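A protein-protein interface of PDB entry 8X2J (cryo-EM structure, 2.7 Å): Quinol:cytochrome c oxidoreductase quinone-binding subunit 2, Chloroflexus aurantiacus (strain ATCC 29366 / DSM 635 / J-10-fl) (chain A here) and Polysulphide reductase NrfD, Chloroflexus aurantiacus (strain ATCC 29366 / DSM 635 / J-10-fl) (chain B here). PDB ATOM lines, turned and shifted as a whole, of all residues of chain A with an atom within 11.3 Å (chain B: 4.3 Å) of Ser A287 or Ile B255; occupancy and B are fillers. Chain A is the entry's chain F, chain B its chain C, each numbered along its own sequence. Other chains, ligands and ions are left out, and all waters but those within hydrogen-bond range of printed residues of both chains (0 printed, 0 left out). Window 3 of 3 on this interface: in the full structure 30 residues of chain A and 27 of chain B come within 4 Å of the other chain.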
ATOM      1  N   SER A 278      -8.100 -23.224 -13.111  1.00  0.00           N
ATOM      2  CA  SER A 278      -7.214 -22.683 -12.085  1.00  0.00           C
ATOM      3  C   SER A 278      -6.360 -23.778 -11.448  1.00  0.00           C
ATOM      4  O   SER A 278      -5.141 -23.612 -11.288  1.00  0.00           O
ATOM      5  CB  SER A 278      -8.032 -21.941 -11.027  1.00  0.00           C
ATOM      6  OG  SER A 278      -8.697 -22.846 -10.168  1.00  0.00           O
ATOM      7  N   TYR A 279      -6.979 -24.915 -11.099  1.00  0.00           N
ATOM      8  CA  TYR A 279      -6.257 -25.975 -10.409  1.00  0.00           C
ATOM      9  C   TYR A 279      -5.251 -26.670 -11.313  1.00  0.00           C
ATOM     10  O   TYR A 279      -4.205 -27.105 -10.827  1.00  0.00           O
ATOM     11  CB  TYR A 279      -7.223 -27.010  -9.831  1.00  0.00           C
ATOM     12  CG  TYR A 279      -6.491 -28.155  -9.170  1.00  0.00           C
ATOM     13  CD1 TYR A 279      -5.710 -27.936  -8.043  1.00  0.00           C
ATOM     14  CD2 TYR A 279      -6.524 -29.437  -9.709  1.00  0.00           C
ATOM     15  CE1 TYR A 279      -5.014 -28.963  -7.445  1.00  0.00           C
ATOM     16  CE2 TYR A 279      -5.828 -30.475  -9.116  1.00  0.00           C
ATOM     17  CZ  TYR A 279      -5.076 -30.227  -7.986  1.00  0.00           C
ATOM     18  OH  TYR A 279      -4.379 -31.244  -7.385  1.00  0.00           O
ATOM     19  N   GLY A 280      -5.542 -26.791 -12.613  1.00  0.00           N
ATOM     20  CA  GLY A 280      -4.589 -27.414 -13.520  1.00  0.00           C
ATOM     21  C   GLY A 280      -3.299 -26.628 -13.635  1.00  0.00           C
ATOM     22  O   GLY A 280      -2.208 -27.193 -13.521  1.00  0.00           O
ATOM     23  N   GLN A 281      -3.416 -25.307 -13.793  1.00  0.00           N
ATOM     24  CA  GLN A 281      -2.256 -24.422 -13.801  1.00  0.00           C
ATOM     25  C   GLN A 281      -1.516 -24.456 -12.472  1.00  0.00           C
ATOM     26  O   GLN A 281      -0.277 -24.511 -12.448  1.00  0.00           O
ATOM     27  CB  GLN A 281      -2.707 -23.000 -14.120  1.00  0.00           C
ATOM     28  CG  GLN A 281      -1.640 -21.941 -13.979  1.00  0.00           C
ATOM     29  CD  GLN A 281      -2.214 -20.545 -13.998  1.00  0.00           C
ATOM     30  OE1 GLN A 281      -3.402 -20.353 -14.252  1.00  0.00           O
ATOM     31  NE2 GLN A 281      -1.376 -19.561 -13.724  1.00  0.00           N
ATOM     32  N   LEU A 282      -2.264 -24.457 -11.362  1.00  0.00           N
ATOM     33  CA  LEU A 282      -1.644 -24.477 -10.041  1.00  0.00           C
ATOM     34  C   LEU A 282      -0.872 -25.769  -9.800  1.00  0.00           C
ATOM     35  O   LEU A 282       0.266 -25.733  -9.329  1.00  0.00           O
ATOM     36  CB  LEU A 282      -2.707 -24.280  -8.965  1.00  0.00           C
ATOM     37  CG  LEU A 282      -2.329 -24.697  -7.546  1.00  0.00           C
ATOM     38  CD1 LEU A 282      -1.300 -23.760  -6.936  1.00  0.00           C
ATOM     39  CD2 LEU A 282      -3.567 -24.731  -6.718  1.00  0.00           C
ATOM     40  N   VAL A 283      -1.461 -26.918 -10.142  1.00  0.00           N
ATOM     41  CA  VAL A 283      -0.788 -28.186  -9.882  1.00  0.00           C
ATOM     42  C   VAL A 283       0.373 -28.393 -10.849  1.00  0.00           C
ATOM     43  O   VAL A 283       1.388 -28.984 -10.468  1.00  0.00           O
ATOM     44  CB  VAL A 283      -1.795 -29.363  -9.886  1.00  0.00           C
ATOM     45  CG1 VAL A 283      -2.281 -29.722 -11.281  1.00  0.00           C
ATOM     46  CG2 VAL A 283      -1.199 -30.588  -9.203  1.00  0.00           C
ATOM     47  N   ILE A 284       0.293 -27.850 -12.071  1.00  0.00           N
ATOM     48  CA  ILE A 284       1.401 -27.975 -13.014  1.00  0.00           C
ATOM     49  C   ILE A 284       2.596 -27.150 -12.547  1.00  0.00           C
ATOM     50  O   ILE A 284       3.726 -27.649 -12.489  1.00  0.00           O
ATOM     51  CB  ILE A 284       0.939 -27.585 -14.430  1.00  0.00           C
ATOM     52  CG1 ILE A 284       0.225 -28.770 -15.067  1.00  0.00           C
ATOM     53  CG2 ILE A 284       2.104 -27.178 -15.311  1.00  0.00           C
ATOM     54  CD1 ILE A 284      -0.716 -28.429 -16.180  1.00  0.00           C
ATOM     55  N   ILE A 285       2.352 -25.897 -12.154  1.00  0.00           N
ATOM     56  CA  ILE A 285       3.433 -25.039 -11.681  1.00  0.00           C
ATOM     57  C   ILE A 285       3.957 -25.504 -10.320  1.00  0.00           C
ATOM     58  O   ILE A 285       5.165 -25.445 -10.058  1.00  0.00           O
ATOM     59  CB  ILE A 285       2.937 -23.579 -11.682  1.00  0.00           C
ATOM     60  CG1 ILE A 285       2.680 -23.134 -13.126  1.00  0.00           C
ATOM     61  CG2 ILE A 285       3.922 -22.634 -11.011  1.00  0.00           C
ATOM     62  CD1 ILE A 285       2.114 -21.743 -13.266  1.00  0.00           C
ATOM     63  N   TRP A 286       3.082 -26.024  -9.456  1.00  0.00           N
ATOM     64  CA  TRP A 286       3.491 -26.474  -8.130  1.00  0.00           C
ATOM     65  C   TRP A 286       4.305 -27.760  -8.202  1.00  0.00           C
ATOM     66  O   TRP A 286       5.338 -27.881  -7.533  1.00  0.00           O
ATOM     67  CB  TRP A 286       2.245 -26.660  -7.262  1.00  0.00           C
ATOM     68  CG  TRP A 286       2.484 -27.085  -5.841  1.00  0.00           C
ATOM     69  CD1 TRP A 286       2.776 -26.278  -4.784  1.00  0.00           C
ATOM     70  CD2 TRP A 286       2.417 -28.419  -5.321  1.00  0.00           C
ATOM     71  NE1 TRP A 286       2.908 -27.025  -3.641  1.00  0.00           N
ATOM     72  CE2 TRP A 286       2.694 -28.344  -3.945  1.00  0.00           C
ATOM     73  CE3 TRP A 286       2.160 -29.668  -5.890  1.00  0.00           C
ATOM     74  CZ2 TRP A 286       2.718 -29.469  -3.129  1.00  0.00           C
ATOM     75  CZ3 TRP A 286       2.186 -30.783  -5.077  1.00  0.00           C
ATOM     76  CH2 TRP A 286       2.464 -30.677  -3.712  1.00  0.00           C
ATOM     77  N   SER A 287       3.862 -28.734  -9.003  1.00  0.00           N
ATOM     78  CA  SER A 287       4.567 -30.002  -9.105  1.00  0.00           C
ATOM     79  C   SER A 287       5.840 -29.877  -9.932  1.00  0.00           C
ATOM     80  O   SER A 287       6.873 -30.448  -9.568  1.00  0.00           O
ATOM     81  CB  SER A 287       3.644 -31.058  -9.702  1.00  0.00           C
ATOM     82  OG  SER A 287       2.394 -31.078  -9.039  1.00  0.00           O
ATOM     83  N   GLY A 288       5.794 -29.145 -11.043  1.00  0.00           N
ATOM     84  CA  GLY A 288       7.016 -28.869 -11.767  1.00  0.00           C
ATOM     85  C   GLY A 288       7.669 -27.622 -11.216  1.00  0.00           C
ATOM     86  O   GLY A 288       7.335 -26.505 -11.618  1.00  0.00           O
ATOM     87  N   ASP A 289       8.625 -27.804 -10.307  1.00  0.00           N
ATOM     88  CA  ASP A 289       9.196 -26.701  -9.537  1.00  0.00           C
ATOM     89  C   ASP A 289      10.275 -25.994 -10.358  1.00  0.00           C
ATOM     90  O   ASP A 289      11.478 -26.109 -10.119  1.00  0.00           O
ATOM     91  CB  ASP A 289       9.742 -27.223  -8.216  1.00  0.00           C
ATOM     92  CG  ASP A 289       9.788 -26.163  -7.144  1.00  0.00           C
ATOM     93  OD1 ASP A 289       8.981 -25.216  -7.211  1.00  0.00           O
ATOM     94  OD2 ASP A 289      10.625 -26.287  -6.227  1.00  0.00           O
ATOM     95  N   VAL A 290       9.816 -25.235 -11.346  1.00  0.00           N
ATOM     96  CA  VAL A 290      10.687 -24.459 -12.220  1.00  0.00           C
ATOM     97  C   VAL A 290      10.589 -23.000 -11.802  1.00  0.00           C
ATOM     98  O   VAL A 290       9.487 -22.474 -11.610  1.00  0.00           O
ATOM     99  CB  VAL A 290      10.300 -24.641 -13.697  1.00  0.00           C
ATOM    100  CG1 VAL A 290      11.357 -24.044 -14.609  1.00  0.00           C
ATOM    101  CG2 VAL A 290      10.085 -26.107 -14.013  1.00  0.00           C
ATOM    102  N   ALA A 291      11.740 -22.338 -11.671  1.00  0.00           N
ATOM    103  CA  ALA A 291      11.777 -20.959 -11.196  1.00  0.00           C
ATOM    104  C   ALA A 291      11.317 -19.949 -12.236  1.00  0.00           C
ATOM    105  O   ALA A 291      11.261 -18.757 -11.921  1.00  0.00           O
ATOM    106  CB  ALA A 291      13.183 -20.602 -10.724  1.00  0.00           C
ATOM    107  N   PHE A 293       8.292 -20.210 -13.408  1.00  0.00           N
ATOM    108  CA  PHE A 293       6.849 -20.222 -13.216  1.00  0.00           C
ATOM    109  C   PHE A 293       6.404 -20.006 -11.780  1.00  0.00           C
ATOM    110  O   PHE A 293       5.353 -19.402 -11.563  1.00  0.00           O
ATOM    111  CB  PHE A 293       6.262 -21.550 -13.706  1.00  0.00           C
ATOM    112  CG  PHE A 293       6.654 -21.897 -15.101  1.00  0.00           C
ATOM    113  CD1 PHE A 293       6.206 -21.134 -16.163  1.00  0.00           C
ATOM    114  CD2 PHE A 293       7.473 -22.985 -15.356  1.00  0.00           C
ATOM    115  CE1 PHE A 293       6.562 -21.449 -17.444  1.00  0.00           C
ATOM    116  CE2 PHE A 293       7.837 -23.305 -16.644  1.00  0.00           C
ATOM    117  CZ  PHE A 293       7.381 -22.536 -17.689  1.00  0.00           C
ATOM    118  N   THR A 294       7.152 -20.498 -10.806  1.00  0.00           N
ATOM    119  CA  THR A 294       6.840 -20.369  -9.384  1.00  0.00           C
ATOM    120  C   THR A 294       6.767 -18.955  -8.780  1.00  0.00           C
ATOM    121  O   THR A 294       6.068 -18.805  -7.766  1.00  0.00           O
ATOM    122  CB  THR A 294       7.839 -21.212  -8.585  1.00  0.00           C
ATOM    123  OG1 THR A 294       9.173 -20.929  -9.019  1.00  0.00           O
ATOM    124  CG2 THR A 294       7.568 -22.683  -8.813  1.00  0.00           C
ATOM    125  N   TYR A 297       2.930 -17.818  -8.303  1.00  0.00           N
ATOM    126  CA  TYR A 297       2.233 -18.264  -7.108  1.00  0.00           C
ATOM    127  C   TYR A 297       2.913 -17.805  -5.827  1.00  0.00           C
ATOM    128  O   TYR A 297       2.252 -17.736  -4.784  1.00  0.00           O
ATOM    129  CB  TYR A 297       2.081 -19.782  -7.144  1.00  0.00           C
ATOM    130  CG  TYR A 297       0.933 -20.191  -8.031  1.00  0.00           C
ATOM    131  CD1 TYR A 297      -0.379 -20.044  -7.604  1.00  0.00           C
ATOM    132  CD2 TYR A 297       1.157 -20.668  -9.318  1.00  0.00           C
ATOM    133  CE1 TYR A 297      -1.436 -20.392  -8.418  1.00  0.00           C
ATOM    134  CE2 TYR A 297       0.105 -21.019 -10.142  1.00  0.00           C
ATOM    135  CZ  TYR A 297      -1.188 -20.878  -9.684  1.00  0.00           C
ATOM    136  OH  TYR A 297      -2.246 -21.221 -10.491  1.00  0.00           O
ATOM    137  N   SER B 166       3.021 -38.209  -7.176  1.00  0.00           N
ATOM    138  CA  SER B 166       3.231 -38.467  -8.584  1.00  0.00           C
ATOM    139  C   SER B 166       1.898 -38.540  -9.307  1.00  0.00           C
ATOM    140  O   SER B 166       0.854 -38.834  -8.721  1.00  0.00           O
ATOM    141  CB  SER B 166       3.968 -39.783  -8.783  1.00  0.00           C
ATOM    142  OG  SER B 166       3.047 -40.842  -8.640  1.00  0.00           O
ATOM    143  N   ALA B 167       1.944 -38.297 -10.611  1.00  0.00           N
ATOM    144  CA  ALA B 167       0.732 -38.378 -11.403  1.00  0.00           C
ATOM    145  C   ALA B 167       0.383 -39.799 -11.814  1.00  0.00           C
ATOM    146  O   ALA B 167      -0.733 -40.031 -12.278  1.00  0.00           O
ATOM    147  CB  ALA B 167       0.860 -37.492 -12.635  1.00  0.00           C
ATOM    148  N   TRP B 170      -2.298 -40.984  -9.453  1.00  0.00           N
ATOM    149  CA  TRP B 170      -3.542 -40.403  -9.944  1.00  0.00           C
ATOM    150  C   TRP B 170      -4.023 -41.144 -11.182  1.00  0.00           C
ATOM    151  O   TRP B 170      -5.226 -41.270 -11.406  1.00  0.00           O
ATOM    152  CB  TRP B 170      -3.382 -38.917 -10.292  1.00  0.00           C
ATOM    153  CG  TRP B 170      -2.547 -38.020  -9.411  1.00  0.00           C
ATOM    154  CD1 TRP B 170      -2.193 -38.208  -8.104  1.00  0.00           C
ATOM    155  CD2 TRP B 170      -1.986 -36.764  -9.797  1.00  0.00           C
ATOM    156  NE1 TRP B 170      -1.432 -37.155  -7.666  1.00  0.00           N
ATOM    157  CE2 TRP B 170      -1.295 -36.253  -8.687  1.00  0.00           C
ATOM    158  CE3 TRP B 170      -2.000 -36.023 -10.982  1.00  0.00           C
ATOM    159  CZ2 TRP B 170      -0.620 -35.040  -8.729  1.00  0.00           C
ATOM    160  CZ3 TRP B 170      -1.327 -34.821 -11.017  1.00  0.00           C
ATOM    161  CH2 TRP B 170      -0.650 -34.339  -9.898  1.00  0.00           C
ATOM    162  N   LEU B 251      -1.391 -34.820 -17.105  1.00  0.00           N
ATOM    163  CA  LEU B 251      -0.550 -34.438 -15.983  1.00  0.00           C
ATOM    164  C   LEU B 251       0.631 -35.371 -15.800  1.00  0.00           C
ATOM    165  O   LEU B 251       1.643 -34.942 -15.244  1.00  0.00           O
ATOM    166  CB  LEU B 251      -1.379 -34.379 -14.702  1.00  0.00           C
ATOM    167  CG  LEU B 251      -2.112 -33.052 -14.505  1.00  0.00           C
ATOM    168  CD1 LEU B 251      -3.313 -33.208 -13.586  1.00  0.00           C
ATOM    169  CD2 LEU B 251      -1.175 -31.996 -14.002  1.00  0.00           C
ATOM    170  N   PHE B 253       2.690 -36.099 -17.954  1.00  0.00           N
ATOM    171  CA  PHE B 253       3.776 -35.326 -18.527  1.00  0.00           C
ATOM    172  C   PHE B 253       3.876 -33.942 -17.913  1.00  0.00           C
ATOM    173  O   PHE B 253       4.978 -33.472 -17.639  1.00  0.00           O
ATOM    174  CB  PHE B 253       3.593 -35.204 -20.044  1.00  0.00           C
ATOM    175  CG  PHE B 253       3.078 -36.455 -20.687  1.00  0.00           C
ATOM    176  CD1 PHE B 253       3.901 -37.559 -20.834  1.00  0.00           C
ATOM    177  CD2 PHE B 253       1.768 -36.537 -21.126  1.00  0.00           C
ATOM    178  CE1 PHE B 253       3.433 -38.718 -21.417  1.00  0.00           C
ATOM    179  CE2 PHE B 253       1.294 -37.695 -21.713  1.00  0.00           C
ATOM    180  CZ  PHE B 253       2.128 -38.786 -21.854  1.00  0.00           C
ATOM    181  N   ALA B 254       2.738 -33.308 -17.622  1.00  0.00           N
ATOM    182  CA  ALA B 254       2.731 -31.896 -17.258  1.00  0.00           C
ATOM    183  C   ALA B 254       3.250 -31.617 -15.849  1.00  0.00           C
ATOM    184  O   ALA B 254       3.586 -30.466 -15.556  1.00  0.00           O
ATOM    185  CB  ALA B 254       1.320 -31.342 -17.427  1.00  0.00           C
ATOM    186  N   ILE B 255       3.335 -32.622 -14.970  1.00  0.00           N
ATOM    187  CA  ILE B 255       3.949 -32.397 -13.662  1.00  0.00           C
ATOM    188  C   ILE B 255       5.460 -32.531 -13.703  1.00  0.00           C
ATOM    189  O   ILE B 255       6.127 -32.258 -12.699  1.00  0.00           O
ATOM    190  CB  ILE B 255       3.438 -33.353 -12.566  1.00  0.00           C
ATOM    191  CG1 ILE B 255       3.880 -34.791 -12.830  1.00  0.00           C
ATOM    192  CG2 ILE B 255       1.936 -33.244 -12.403  1.00  0.00           C
ATOM    193  CD1 ILE B 255       3.992 -35.629 -11.578  1.00  0.00           C
ATOM    194  N   SER B 256       6.016 -32.953 -14.831  1.00  0.00           N
ATOM    195  CA  SER B 256       7.449 -33.104 -14.975  1.00  0.00           C
ATOM    196  C   SER B 256       8.089 -31.782 -15.382  1.00  0.00           C
ATOM    197  O   SER B 256       7.425 -30.847 -15.828  1.00  0.00           O
ATOM    198  CB  SER B 256       7.767 -34.179 -16.005  1.00  0.00           C
ATOM    199  OG  SER B 256       7.719 -33.627 -17.305  1.00  0.00           O
ATOM    200  N   GLN B 257       9.408 -31.720 -15.237  1.00  0.00           N
ATOM    201  CA  GLN B 257      10.180 -30.536 -15.576  1.00  0.00           C
ATOM    202  C   GLN B 257      10.723 -30.573 -16.997  1.00  0.00           C
ATOM    203  O   GLN B 257      11.529 -29.710 -17.353  1.00  0.00           O
ATOM    204  CB  GLN B 257      11.331 -30.366 -14.586  1.00  0.00           C
ATOM    205  CG  GLN B 257      10.943 -29.673 -13.300  1.00  0.00           C
ATOM    206  CD  GLN B 257      12.093 -29.582 -12.329  1.00  0.00           C
ATOM    207  OE1 GLN B 257      13.225 -29.924 -12.664  1.00  0.00           O
ATOM    208  NE2 GLN B 257      11.814 -29.116 -11.119  1.00  0.00           N
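The side-chain amide nitrogen (NE2) of Gln B257 is in hydrogen-bond range of the backbone carbonyl oxygen (O) of Asp A289.
O of Ser B166 lies within hydrogen-bond range of NE1 of Trp B170 (3.0 Å).
The backbone carbonyl oxygen (O) of Val A283 is in hydrogen-bond range of the side-chain hydroxyl (OG) of Ser A287 (2.7 Å).
O of Val A290 sits at hydrogen-bond distance from OG1 of Thr A294.
CG2 of Val A283 touches CH2 of Trp B170 (3.9 Å).
CG1 of Val A283 touches CD2 of Leu B251, 3.7 Å away.
Leu B251 touches Ile A284.
O of Ala B254 touches CG2 of Ile A284, 3.6 Å away.
Ile B255 touches Ser A287 (O to C, 3.7 Å).
Gly A288 touches Ile B255.
Gln B257 touches Val A290 (CG to CG2, 3.7 Å).
Of chain B, only Ile B255 comes within 4 Å of Ser A287.
Of chain A, only Ser A287 (3.7 Å) and Gly A288 (3.5 Å) come within 4 Å of Ile B255.
No residue of chain A comes within 4 Å of Ser B166.
No residue of chain A comes within 4 Å of Ala B167.
Leu B251 touches two residues of chain A.
Of the printed residues of chain A, Ala B254 touches Ile A284.
Printed residues of chain B within 4 Å of Gly A288: Ile B255 (3.5 Å).
Printed residues of chain A within 4 Å of Trp B170: Val A283 (3.9 Å).
Gly A280 touches none of the printed residues of chain B.
Leu A282 touches none of the printed residues of chain B.
The nearest printed residue of chain B that does not touch Gly A288 is Gln B257 (4.3 Å).
Of the 9 printed residues of chain B, 5 touch a printed residue of chain A.
Hydrophobic or aromatic side chains of chain A within 4 Å of the printed part of chain B: Val A283, Ile A284 and Val A290.
Among the printed residues, 8 pairs touch across the chains.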
